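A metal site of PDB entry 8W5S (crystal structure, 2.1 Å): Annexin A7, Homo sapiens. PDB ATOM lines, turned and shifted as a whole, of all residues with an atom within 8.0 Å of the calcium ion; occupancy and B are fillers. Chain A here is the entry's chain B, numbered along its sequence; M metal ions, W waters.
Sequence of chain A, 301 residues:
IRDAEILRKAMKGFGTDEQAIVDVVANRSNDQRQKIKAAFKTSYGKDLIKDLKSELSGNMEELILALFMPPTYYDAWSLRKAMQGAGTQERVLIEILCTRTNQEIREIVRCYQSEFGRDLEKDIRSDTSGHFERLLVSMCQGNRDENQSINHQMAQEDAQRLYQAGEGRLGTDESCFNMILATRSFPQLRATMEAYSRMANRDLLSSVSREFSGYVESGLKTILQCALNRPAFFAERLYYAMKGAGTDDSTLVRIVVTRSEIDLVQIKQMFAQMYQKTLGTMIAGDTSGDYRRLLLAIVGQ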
ATOM      1  N   LYS A 122      21.549  23.772  -2.218  1.00  0.00           N
ATOM      2  CA  LYS A 122      21.412  24.299  -3.571  1.00  0.00           C
ATOM      3  C   LYS A 122      21.050  23.199  -4.560  1.00  0.00           C
ATOM      4  O   LYS A 122      20.139  23.364  -5.388  1.00  0.00           O
ATOM      5  CB  LYS A 122      22.698  24.999  -3.995  1.00  0.00           C
ATOM      6  CG  LYS A 122      22.679  26.511  -3.827  1.00  0.00           C
ATOM      7  CD  LYS A 122      23.685  27.182  -4.743  1.00  0.00           C
ATOM      8  CE  LYS A 122      25.115  26.995  -4.254  1.00  0.00           C
ATOM      9  NZ  LYS A 122      25.432  27.909  -3.123  1.00  0.00           N
ATOM     10  N   ASP A 123      21.738  22.058  -4.480  1.00  0.00           N
ATOM     11  CA  ASP A 123      21.490  20.967  -5.410  1.00  0.00           C
ATOM     12  C   ASP A 123      20.055  20.456  -5.303  1.00  0.00           C
ATOM     13  O   ASP A 123      19.466  20.052  -6.307  1.00  0.00           O
ATOM     14  CB  ASP A 123      22.464  19.820  -5.140  1.00  0.00           C
ATOM     15  CG  ASP A 123      23.892  20.181  -5.506  1.00  0.00           C
ATOM     16  OD1 ASP A 123      24.095  21.241  -6.135  1.00  0.00           O
ATOM     17  OD2 ASP A 123      24.809  19.412  -5.150  1.00  0.00           O
ATOM     18  N   ILE A 124      19.484  20.470  -4.100  1.00  0.00           N
ATOM     19  CA  ILE A 124      18.099  20.038  -3.926  1.00  0.00           C
ATOM     20  C   ILE A 124      17.152  20.997  -4.631  1.00  0.00           C
ATOM     21  O   ILE A 124      16.219  20.577  -5.326  1.00  0.00           O
ATOM     22  CB  ILE A 124      17.762  19.905  -2.435  1.00  0.00           C
ATOM     23  CG1 ILE A 124      18.228  18.547  -1.906  1.00  0.00           C
ATOM     24  CG2 ILE A 124      16.266  20.083  -2.194  1.00  0.00           C
ATOM     25  CD1 ILE A 124      18.220  18.461  -0.412  1.00  0.00           C
ATOM     26  N   ARG A 125      17.393  22.304  -4.462  1.00  0.00           N
ATOM     27  CA  ARG A 125      16.527  23.318  -5.063  1.00  0.00           C
ATOM     28  C   ARG A 125      16.428  23.141  -6.574  1.00  0.00           C
ATOM     29  O   ARG A 125      15.349  23.296  -7.155  1.00  0.00           O
ATOM     30  CB  ARG A 125      17.057  24.706  -4.738  1.00  0.00           C
ATOM     31  CG  ARG A 125      16.660  25.198  -3.353  1.00  0.00           C
ATOM     32  CD  ARG A 125      16.258  26.665  -3.389  1.00  0.00           C
ATOM     33  NE  ARG A 125      16.246  27.240  -2.045  1.00  0.00           N
ATOM     34  CZ  ARG A 125      15.150  27.373  -1.309  1.00  0.00           C
ATOM     35  NH1 ARG A 125      13.958  27.008  -1.766  1.00  0.00           N
ATOM     36  NH2 ARG A 125      15.250  27.901  -0.087  1.00  0.00           N
ATOM     37  N   SER A 126      17.539  22.810  -7.228  1.00  0.00           N
ATOM     38  CA  SER A 126      17.533  22.633  -8.672  1.00  0.00           C
ATOM     39  C   SER A 126      17.084  21.251  -9.106  1.00  0.00           C
ATOM     40  O   SER A 126      16.805  21.043 -10.290  1.00  0.00           O
ATOM     41  CB  SER A 126      18.936  22.922  -9.232  1.00  0.00           C
ATOM     42  OG  SER A 126      19.903  22.084  -8.642  1.00  0.00           O
ATOM     43  N   ASP A 127      16.994  20.287  -8.189  1.00  0.00           N
ATOM     44  CA  ASP A 127      16.533  18.945  -8.525  1.00  0.00           C
ATOM     45  C   ASP A 127      15.078  18.687  -8.127  1.00  0.00           C
ATOM     46  O   ASP A 127      14.449  17.805  -8.712  1.00  0.00           O
ATOM     47  CB  ASP A 127      17.427  17.884  -7.866  1.00  0.00           C
ATOM     48  CG  ASP A 127      18.117  17.012  -8.892  1.00  0.00           C
ATOM     49  OD1 ASP A 127      19.102  17.473  -9.508  1.00  0.00           O
ATOM     50  OD2 ASP A 127      17.684  15.852  -9.079  1.00  0.00           O
ATOM     51  N   THR A 128      14.555  19.413  -7.148  1.00  0.00           N
ATOM     52  CA  THR A 128      13.172  19.289  -6.713  1.00  0.00           C
ATOM     53  C   THR A 128      12.469  20.642  -6.855  1.00  0.00           C
ATOM     54  O   THR A 128      13.096  21.659  -7.158  1.00  0.00           O
ATOM     55  CB  THR A 128      13.091  18.798  -5.255  1.00  0.00           C
ATOM     56  OG1 THR A 128      13.647  19.781  -4.382  1.00  0.00           O
ATOM     57  CG2 THR A 128      13.859  17.492  -5.105  1.00  0.00           C
ATOM     58  N   SER A 129      11.159  20.630  -6.636  1.00  0.00           N
ATOM     59  CA  SER A 129      10.341  21.819  -6.872  1.00  0.00           C
ATOM     60  C   SER A 129       9.071  21.760  -6.035  1.00  0.00           C
ATOM     61  O   SER A 129       8.682  20.699  -5.539  1.00  0.00           O
ATOM     62  CB  SER A 129       9.966  21.954  -8.360  1.00  0.00           C
ATOM     63  OG  SER A 129       9.226  20.837  -8.812  1.00  0.00           O
ATOM     64  N   GLY A 130       8.451  22.922  -5.871  1.00  0.00           N
ATOM     65  CA  GLY A 130       7.123  22.994  -5.283  1.00  0.00           C
ATOM     66  C   GLY A 130       7.151  23.045  -3.759  1.00  0.00           C
ATOM     67  O   GLY A 130       8.058  23.600  -3.144  1.00  0.00           O
ATOM     68  N   GLU A 133      10.066  20.790  -2.512  1.00  0.00           N
ATOM     69  CA  GLU A 133      11.319  21.525  -2.355  1.00  0.00           C
ATOM     70  C   GLU A 133      11.315  22.327  -1.049  1.00  0.00           C
ATOM     71  O   GLU A 133      12.343  22.386  -0.363  1.00  0.00           O
ATOM     72  CB  GLU A 133      11.552  22.448  -3.551  1.00  0.00           C
ATOM     73  CG  GLU A 133      12.828  23.265  -3.464  1.00  0.00           C
ATOM     74  CD  GLU A 133      12.892  24.356  -4.523  1.00  0.00           C
ATOM     75  OE1 GLU A 133      12.877  24.024  -5.719  1.00  0.00           O
ATOM     76  OE2 GLU A 133      12.984  25.544  -4.141  1.00  0.00           O
HETATM   77 CA    CA M   1      13.378  23.918  -8.239  1.00  0.00          CA
HETATM   78  O   HOH W   1      10.820  24.971  -7.825  1.00  0.00           O
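The side-chain hydroxyl (OG1) of Thr 128 sits at hydrogen-bond distance from the backbone carbonyl oxygen (O) of Ile 124 (2.9 Å).
CA of Ser 129 touches the calcium ion, at 3.9 Å. Four residues have an atom within 4 Å of the calcium ion: Arg 125, Thr 128, Ser 129 and Glu 133.
The calcium ion is bound by the backbone carbonyl oxygen of Arg 125 (2.3 Å), the backbone carbonyl oxygen of Thr 128 (2.5 Å), the side-chain carboxylate of Glu 133 (2.6 Å) and water W1 (2.8 Å). The calcium ion has four donor atoms within binding distance.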
